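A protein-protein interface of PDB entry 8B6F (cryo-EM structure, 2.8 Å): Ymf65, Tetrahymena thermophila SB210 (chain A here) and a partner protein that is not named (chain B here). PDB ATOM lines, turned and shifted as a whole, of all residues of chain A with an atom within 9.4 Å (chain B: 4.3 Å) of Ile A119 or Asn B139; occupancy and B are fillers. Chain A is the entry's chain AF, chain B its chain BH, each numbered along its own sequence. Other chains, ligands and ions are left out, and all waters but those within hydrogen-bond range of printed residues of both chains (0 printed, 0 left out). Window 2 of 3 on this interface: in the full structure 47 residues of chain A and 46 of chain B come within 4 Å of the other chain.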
ATOM      1  N   ASN A  55      10.964  -8.190 -32.389  1.00  0.00           N
ATOM      2  CA  ASN A  55      11.049  -7.089 -31.446  1.00  0.00           C
ATOM      3  C   ASN A  55       9.642  -6.651 -31.043  1.00  0.00           C
ATOM      4  O   ASN A  55       8.754  -6.555 -31.897  1.00  0.00           O
ATOM      5  CB  ASN A  55      11.814  -5.923 -32.070  1.00  0.00           C
ATOM      6  CG  ASN A  55      12.044  -4.789 -31.097  1.00  0.00           C
ATOM      7  OD1 ASN A  55      11.103  -4.257 -30.511  1.00  0.00           O
ATOM      8  ND2 ASN A  55      13.303  -4.410 -30.918  1.00  0.00           N
ATOM      9  N   SER A  57       8.491  -3.812 -30.337  1.00  0.00           N
ATOM     10  CA  SER A  57       8.205  -2.404 -30.579  1.00  0.00           C
ATOM     11  C   SER A  57       6.798  -2.212 -31.132  1.00  0.00           C
ATOM     12  O   SER A  57       6.122  -1.233 -30.798  1.00  0.00           O
ATOM     13  CB  SER A  57       9.241  -1.822 -31.539  1.00  0.00           C
ATOM     14  OG  SER A  57       8.990  -0.452 -31.793  1.00  0.00           O
ATOM     15  N   ILE A  60       4.315  -2.448 -28.284  1.00  0.00           N
ATOM     16  CA  ILE A  60       4.337  -1.233 -27.474  1.00  0.00           C
ATOM     17  C   ILE A  60       3.627  -0.101 -28.202  1.00  0.00           C
ATOM     18  O   ILE A  60       2.880   0.677 -27.596  1.00  0.00           O
ATOM     19  CB  ILE A  60       5.787  -0.856 -27.121  1.00  0.00           C
ATOM     20  CG1 ILE A  60       6.476  -2.009 -26.395  1.00  0.00           C
ATOM     21  CG2 ILE A  60       5.809   0.386 -26.245  1.00  0.00           C
ATOM     22  CD1 ILE A  60       7.969  -1.833 -26.263  1.00  0.00           C
ATOM     23  N   TYR A 111       5.999   5.201 -23.996  1.00  0.00           N
ATOM     24  CA  TYR A 111       6.812   5.859 -25.012  1.00  0.00           C
ATOM     25  C   TYR A 111       8.299   5.715 -24.703  1.00  0.00           C
ATOM     26  O   TYR A 111       9.096   5.376 -25.585  1.00  0.00           O
ATOM     27  CB  TYR A 111       6.411   7.334 -25.105  1.00  0.00           C
ATOM     28  CG  TYR A 111       7.181   8.134 -26.128  1.00  0.00           C
ATOM     29  CD1 TYR A 111       6.853   8.079 -27.475  1.00  0.00           C
ATOM     30  CD2 TYR A 111       8.215   8.973 -25.739  1.00  0.00           C
ATOM     31  CE1 TYR A 111       7.548   8.820 -28.410  1.00  0.00           C
ATOM     32  CE2 TYR A 111       8.917   9.716 -26.665  1.00  0.00           C
ATOM     33  CZ  TYR A 111       8.578   9.637 -27.997  1.00  0.00           C
ATOM     34  OH  TYR A 111       9.275  10.378 -28.921  1.00  0.00           O
ATOM     35  N   ILE A 112       8.692   5.974 -23.456  1.00  0.00           N
ATOM     36  CA  ILE A 112      10.096   5.832 -23.073  1.00  0.00           C
ATOM     37  C   ILE A 112      10.546   4.387 -23.236  1.00  0.00           C
ATOM     38  O   ILE A 112      11.661   4.111 -23.696  1.00  0.00           O
ATOM     39  CB  ILE A 112      10.308   6.329 -21.631  1.00  0.00           C
ATOM     40  CG1 ILE A 112       9.824   7.774 -21.478  1.00  0.00           C
ATOM     41  CG2 ILE A 112      11.771   6.199 -21.225  1.00  0.00           C
ATOM     42  CD1 ILE A 112      10.482   8.754 -22.418  1.00  0.00           C
ATOM     43  N   THR A 113       9.686   3.444 -22.858  1.00  0.00           N
ATOM     44  CA  THR A 113      10.009   2.028 -22.984  1.00  0.00           C
ATOM     45  C   THR A 113      10.199   1.627 -24.438  1.00  0.00           C
ATOM     46  O   THR A 113      11.079   0.819 -24.757  1.00  0.00           O
ATOM     47  CB  THR A 113       8.913   1.204 -22.323  1.00  0.00           C
ATOM     48  OG1 THR A 113       8.877   1.540 -20.934  1.00  0.00           O
ATOM     49  CG2 THR A 113       9.177  -0.284 -22.483  1.00  0.00           C
ATOM     50  N   GLU A 114       9.384   2.177 -25.335  1.00  0.00           N
ATOM     51  CA  GLU A 114       9.557   1.887 -26.751  1.00  0.00           C
ATOM     52  C   GLU A 114      10.926   2.346 -27.227  1.00  0.00           C
ATOM     53  O   GLU A 114      11.609   1.625 -27.962  1.00  0.00           O
ATOM     54  CB  GLU A 114       8.451   2.562 -27.560  1.00  0.00           C
ATOM     55  CG  GLU A 114       8.573   2.360 -29.055  1.00  0.00           C
ATOM     56  CD  GLU A 114       7.487   3.083 -29.820  1.00  0.00           C
ATOM     57  OE1 GLU A 114       6.496   3.501 -29.189  1.00  0.00           O
ATOM     58  OE2 GLU A 114       7.628   3.243 -31.050  1.00  0.00           O
ATOM     59  N   LYS A 115      11.342   3.547 -26.829  1.00  0.00           N
ATOM     60  CA  LYS A 115      12.670   4.020 -27.196  1.00  0.00           C
ATOM     61  C   LYS A 115      13.748   3.091 -26.652  1.00  0.00           C
ATOM     62  O   LYS A 115      14.701   2.752 -27.362  1.00  0.00           O
ATOM     63  CB  LYS A 115      12.878   5.442 -26.675  1.00  0.00           C
ATOM     64  CG  LYS A 115      11.839   6.438 -27.165  1.00  0.00           C
ATOM     65  CD  LYS A 115      11.782   6.503 -28.676  1.00  0.00           C
ATOM     66  CE  LYS A 115      10.729   7.490 -29.135  1.00  0.00           C
ATOM     67  NZ  LYS A 115      10.626   7.521 -30.617  1.00  0.00           N
ATOM     68  N   HIS A 116      13.620   2.673 -25.390  1.00  0.00           N
ATOM     69  CA  HIS A 116      14.619   1.786 -24.799  1.00  0.00           C
ATOM     70  C   HIS A 116      14.677   0.448 -25.525  1.00  0.00           C
ATOM     71  O   HIS A 116      15.762  -0.099 -25.747  1.00  0.00           O
ATOM     72  CB  HIS A 116      14.329   1.565 -23.316  1.00  0.00           C
ATOM     73  CG  HIS A 116      15.220   0.544 -22.683  1.00  0.00           C
ATOM     74  ND1 HIS A 116      14.760  -0.679 -22.244  1.00  0.00           N
ATOM     75  CD2 HIS A 116      16.550   0.556 -22.434  1.00  0.00           C
ATOM     76  CE1 HIS A 116      15.767  -1.372 -21.745  1.00  0.00           C
ATOM     77  NE2 HIS A 116      16.865  -0.646 -21.848  1.00  0.00           N
ATOM     78  N   ILE A 117      13.521  -0.096 -25.898  1.00  0.00           N
ATOM     79  CA  ILE A 117      13.492  -1.380 -26.592  1.00  0.00           C
ATOM     80  C   ILE A 117      14.167  -1.269 -27.951  1.00  0.00           C
ATOM     81  O   ILE A 117      14.900  -2.172 -28.371  1.00  0.00           O
ATOM     82  CB  ILE A 117      12.045  -1.897 -26.702  1.00  0.00           C
ATOM     83  CG1 ILE A 117      11.543  -2.307 -25.315  1.00  0.00           C
ATOM     84  CG2 ILE A 117      11.944  -3.049 -27.700  1.00  0.00           C
ATOM     85  CD1 ILE A 117      12.178  -3.579 -24.779  1.00  0.00           C
ATOM     86  N   LYS A 118      13.927  -0.171 -28.663  1.00  0.00           N
ATOM     87  CA  LYS A 118      14.660   0.062 -29.903  1.00  0.00           C
ATOM     88  C   LYS A 118      16.163   0.089 -29.648  1.00  0.00           C
ATOM     89  O   LYS A 118      16.946  -0.406 -30.467  1.00  0.00           O
ATOM     90  CB  LYS A 118      14.195   1.374 -30.538  1.00  0.00           C
ATOM     91  CG  LYS A 118      12.802   1.305 -31.154  1.00  0.00           C
ATOM     92  CD  LYS A 118      12.297   2.692 -31.523  1.00  0.00           C
ATOM     93  CE  LYS A 118      10.845   2.650 -31.959  1.00  0.00           C
ATOM     94  NZ  LYS A 118      10.259   4.018 -32.015  1.00  0.00           N
ATOM     95  N   ILE A 119      16.588   0.654 -28.513  1.00  0.00           N
ATOM     96  CA  ILE A 119      18.009   0.638 -28.168  1.00  0.00           C
ATOM     97  C   ILE A 119      18.501  -0.797 -28.034  1.00  0.00           C
ATOM     98  O   ILE A 119      19.507  -1.188 -28.635  1.00  0.00           O
ATOM     99  CB  ILE A 119      18.261   1.424 -26.869  1.00  0.00           C
ATOM    100  CG1 ILE A 119      17.947   2.905 -27.058  1.00  0.00           C
ATOM    101  CG2 ILE A 119      19.709   1.258 -26.409  1.00  0.00           C
ATOM    102  CD1 ILE A 119      17.935   3.661 -25.762  1.00  0.00           C
ATOM    103  N   LEU A 120      17.794  -1.601 -27.244  1.00  0.00           N
ATOM    104  CA  LEU A 120      18.213  -2.972 -26.993  1.00  0.00           C
ATOM    105  C   LEU A 120      17.001  -3.788 -26.571  1.00  0.00           C
ATOM    106  O   LEU A 120      16.105  -3.288 -25.889  1.00  0.00           O
ATOM    107  CB  LEU A 120      19.300  -3.030 -25.916  1.00  0.00           C
ATOM    108  CG  LEU A 120      19.842  -4.422 -25.588  1.00  0.00           C
ATOM    109  CD1 LEU A 120      20.493  -5.046 -26.811  1.00  0.00           C
ATOM    110  CD2 LEU A 120      20.826  -4.344 -24.434  1.00  0.00           C
ATOM    111  N   ASN A 121      16.996  -5.057 -26.974  1.00  0.00           N
ATOM    112  CA  ASN A 121      15.858  -5.953 -26.782  1.00  0.00           C
ATOM    113  C   ASN A 121      16.264  -7.090 -25.852  1.00  0.00           C
ATOM    114  O   ASN A 121      16.932  -8.039 -26.276  1.00  0.00           O
ATOM    115  CB  ASN A 121      15.365  -6.484 -28.125  1.00  0.00           C
ATOM    116  CG  ASN A 121      14.233  -7.479 -27.978  1.00  0.00           C
ATOM    117  OD1 ASN A 121      13.566  -7.531 -26.946  1.00  0.00           O
ATOM    118  ND2 ASN A 121      14.011  -8.278 -29.014  1.00  0.00           N
ATOM    119  N   ASN A 122      15.859  -6.992 -24.585  1.00  0.00           N
ATOM    120  CA  ASN A 122      15.990  -8.085 -23.626  1.00  0.00           C
ATOM    121  C   ASN A 122      14.639  -8.488 -23.050  1.00  0.00           C
ATOM    122  O   ASN A 122      14.583  -9.123 -21.993  1.00  0.00           O
ATOM    123  CB  ASN A 122      16.945  -7.698 -22.494  1.00  0.00           C
ATOM    124  CG  ASN A 122      18.396  -7.699 -22.925  1.00  0.00           C
ATOM    125  OD1 ASN A 122      18.791  -8.447 -23.817  1.00  0.00           O
ATOM    126  ND2 ASN A 122      19.202  -6.861 -22.284  1.00  0.00           N
ATOM    127  N   TYR A 123      13.548  -8.127 -23.721  1.00  0.00           N
ATOM    128  CA  TYR A 123      12.201  -8.339 -23.211  1.00  0.00           C
ATOM    129  C   TYR A 123      11.352  -8.977 -24.299  1.00  0.00           C
ATOM    130  O   TYR A 123      11.392  -8.544 -25.455  1.00  0.00           O
ATOM    131  CB  TYR A 123      11.588  -7.014 -22.750  1.00  0.00           C
ATOM    132  CG  TYR A 123      12.513  -6.217 -21.860  1.00  0.00           C
ATOM    133  CD1 TYR A 123      13.468  -5.365 -22.402  1.00  0.00           C
ATOM    134  CD2 TYR A 123      12.446  -6.330 -20.478  1.00  0.00           C
ATOM    135  CE1 TYR A 123      14.321  -4.641 -21.594  1.00  0.00           C
ATOM    136  CE2 TYR A 123      13.295  -5.612 -19.661  1.00  0.00           C
ATOM    137  CZ  TYR A 123      14.230  -4.769 -20.225  1.00  0.00           C
ATOM    138  OH  TYR A 123      15.078  -4.052 -19.414  1.00  0.00           O
ATOM    139  N   LEU B 131      28.086   2.282 -22.274  1.00  0.00           N
ATOM    140  CA  LEU B 131      27.193   2.330 -23.422  1.00  0.00           C
ATOM    141  C   LEU B 131      27.248   1.023 -24.200  1.00  0.00           C
ATOM    142  O   LEU B 131      28.314   0.424 -24.361  1.00  0.00           O
ATOM    143  CB  LEU B 131      27.563   3.496 -24.340  1.00  0.00           C
ATOM    144  CG  LEU B 131      27.387   4.894 -23.741  1.00  0.00           C
ATOM    145  CD1 LEU B 131      27.911   5.950 -24.694  1.00  0.00           C
ATOM    146  CD2 LEU B 131      25.929   5.165 -23.402  1.00  0.00           C
ATOM    147  N   ASN B 132      26.086   0.578 -24.670  1.00  0.00           N
ATOM    148  CA  ASN B 132      26.027  -0.597 -25.528  1.00  0.00           C
ATOM    149  C   ASN B 132      26.622  -0.279 -26.892  1.00  0.00           C
ATOM    150  O   ASN B 132      26.478   0.831 -27.409  1.00  0.00           O
ATOM    151  CB  ASN B 132      24.584  -1.073 -25.690  1.00  0.00           C
ATOM    152  CG  ASN B 132      24.000  -1.605 -24.400  1.00  0.00           C
ATOM    153  OD1 ASN B 132      23.355  -0.875 -23.650  1.00  0.00           O
ATOM    154  ND2 ASN B 132      24.227  -2.886 -24.134  1.00  0.00           N
ATOM    155  N   LYS B 134      26.771  -0.845 -30.887  1.00  0.00           N
ATOM    156  CA  LYS B 134      25.988  -1.256 -32.041  1.00  0.00           C
ATOM    157  C   LYS B 134      26.689  -0.759 -33.293  1.00  0.00           C
ATOM    158  O   LYS B 134      27.035   0.423 -33.383  1.00  0.00           O
ATOM    159  CB  LYS B 134      24.561  -0.709 -31.970  1.00  0.00           C
ATOM    160  CG  LYS B 134      23.637  -1.250 -33.046  1.00  0.00           C
ATOM    161  CD  LYS B 134      22.213  -0.769 -32.837  1.00  0.00           C
ATOM    162  CE  LYS B 134      21.259  -1.447 -33.801  1.00  0.00           C
ATOM    163  NZ  LYS B 134      19.849  -1.033 -33.565  1.00  0.00           N
ATOM    164  N   TYR B 137      30.096   0.742 -32.645  1.00  0.00           N
ATOM    165  CA  TYR B 137      30.161   2.028 -31.970  1.00  0.00           C
ATOM    166  C   TYR B 137      29.137   2.077 -30.849  1.00  0.00           C
ATOM    167  O   TYR B 137      28.109   1.396 -30.892  1.00  0.00           O
ATOM    168  CB  TYR B 137      29.911   3.189 -32.942  1.00  0.00           C
ATOM    169  CG  TYR B 137      31.098   3.527 -33.811  1.00  0.00           C
ATOM    170  CD1 TYR B 137      32.130   4.318 -33.330  1.00  0.00           C
ATOM    171  CD2 TYR B 137      31.177   3.067 -35.118  1.00  0.00           C
ATOM    172  CE1 TYR B 137      33.215   4.633 -34.123  1.00  0.00           C
ATOM    173  CE2 TYR B 137      32.257   3.377 -35.918  1.00  0.00           C
ATOM    174  CZ  TYR B 137      33.272   4.160 -35.416  1.00  0.00           C
ATOM    175  OH  TYR B 137      34.349   4.471 -36.211  1.00  0.00           O
ATOM    176  N   VAL B 138      29.431   2.895 -29.837  1.00  0.00           N
ATOM    177  CA  VAL B 138      28.510   3.057 -28.723  1.00  0.00           C
ATOM    178  C   VAL B 138      27.187   3.604 -29.230  1.00  0.00           C
ATOM    179  O   VAL B 138      27.144   4.508 -30.074  1.00  0.00           O
ATOM    180  CB  VAL B 138      29.116   3.975 -27.647  1.00  0.00           C
ATOM    181  CG1 VAL B 138      30.315   3.307 -27.004  1.00  0.00           C
ATOM    182  CG2 VAL B 138      29.501   5.325 -28.238  1.00  0.00           C
ATOM    183  N   ASN B 139      26.095   3.053 -28.715  1.00  0.00           N
ATOM    184  CA  ASN B 139      24.751   3.426 -29.134  1.00  0.00           C
ATOM    185  C   ASN B 139      24.207   4.460 -28.155  1.00  0.00           C
ATOM    186  O   ASN B 139      23.903   4.135 -27.002  1.00  0.00           O
ATOM    187  CB  ASN B 139      23.851   2.193 -29.190  1.00  0.00           C
ATOM    188  CG  ASN B 139      22.498   2.484 -29.802  1.00  0.00           C
ATOM    189  OD1 ASN B 139      22.014   3.614 -29.766  1.00  0.00           O
ATOM    190  ND2 ASN B 139      21.873   1.458 -30.362  1.00  0.00           N
ATOM    191  N   ILE B 140      24.083   5.701 -28.618  1.00  0.00           N
ATOM    192  CA  ILE B 140      23.511   6.793 -27.840  1.00  0.00           C
ATOM    193  C   ILE B 140      22.161   7.131 -28.452  1.00  0.00           C
ATOM    194  O   ILE B 140      22.067   7.397 -29.656  1.00  0.00           O
ATOM    195  CB  ILE B 140      24.433   8.023 -27.820  1.00  0.00           C
ATOM    196  CG1 ILE B 140      25.823   7.632 -27.308  1.00  0.00           C
ATOM    197  CG2 ILE B 140      23.828   9.118 -26.950  1.00  0.00           C
ATOM    198  CD1 ILE B 140      26.826   8.766 -27.298  1.00  0.00           C
ATOM    199  N   ASN B 141      21.121   7.122 -27.628  1.00  0.00           N
ATOM    200  CA  ASN B 141      19.748   7.266 -28.100  1.00  0.00           C
ATOM    201  C   ASN B 141      19.333   8.728 -28.005  1.00  0.00           C
ATOM    202  O   ASN B 141      19.199   9.274 -26.908  1.00  0.00           O
ATOM    203  CB  ASN B 141      18.807   6.382 -27.295  1.00  0.00           C
ATOM    204  CG  ASN B 141      17.420   6.317 -27.899  1.00  0.00           C
ATOM    205  OD1 ASN B 141      16.530   7.076 -27.521  1.00  0.00           O
ATOM    206  ND2 ASN B 141      17.230   5.406 -28.844  1.00  0.00           N
ATOM    207  N   ILE B 144      15.892   9.273 -25.992  1.00  0.00           N
ATOM    208  CA  ILE B 144      15.985   9.233 -24.535  1.00  0.00           C
ATOM    209  C   ILE B 144      16.768  10.432 -24.012  1.00  0.00           C
ATOM    210  O   ILE B 144      16.451  10.975 -22.949  1.00  0.00           O
ATOM    211  CB  ILE B 144      16.585   7.896 -24.062  1.00  0.00           C
ATOM    212  CG1 ILE B 144      15.554   6.781 -24.269  1.00  0.00           C
ATOM    213  CG2 ILE B 144      17.043   7.986 -22.604  1.00  0.00           C
ATOM    214  CD1 ILE B 144      15.950   5.441 -23.708  1.00  0.00           C
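Printed residues of chain B that touch a printed residue of chain A: Asn B132, Asn B139, Asn B141 and Ile B144.
Hydrophobic or aromatic side chains of chain B within 4 Å of the printed part of chain A: Ile B144.
Of the 16 printed residues of chain A, 4 touch a printed residue of chain B.
Hydrophobic or aromatic side chains of chain A within 4 Å of the printed part of chain B: Ile A119 and Leu A120.
Along chain A the printed residues that touch a printed residue of chain B span positions 115 to 120.
Among the printed residues, 7 pairs touch across the chains.
Glu A114 touches none of the printed residues of chain B.
Of the printed residues of chain B, Lys A115 touches Asn B141 (3.95 Å) and Ile B144 (3.8 Å).
Of chain B, only Asn B139, Asn B141 and Ile B144 come within 4 Å of Ile A119.
Tyr A123 touches none of the printed residues of chain B.
Of the printed residues of chain A, Asn B132 touches Leu A120 (3.7 Å).
Of chain A, only Ile A119 (3.9 Å) comes within 4 Å of Asn B139.
No residue of chain A comes within 4 Å of Ile B140.
The nearest printed residue of chain A that does not touch Asn B141 is Lys A118 (5.3 Å).
The backbone NH (N) of Ile B144 is in hydrogen-bond range of the side-chain amide oxygen (OD1) of Asn B141.
O of Asn B132 is in hydrogen-bond range of N of Asn B139 (2.6 Å).
Among the printed residues, pairs that only touch across the chains: Ile A119 with Asn B141, Ile A119 with Ile B144, Leu A120 with Asn B132, Lys A115 with Ile B144, Ile A119 with Asn B139, Lys A115 with Asn B141 and His A116 with Ile B144.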
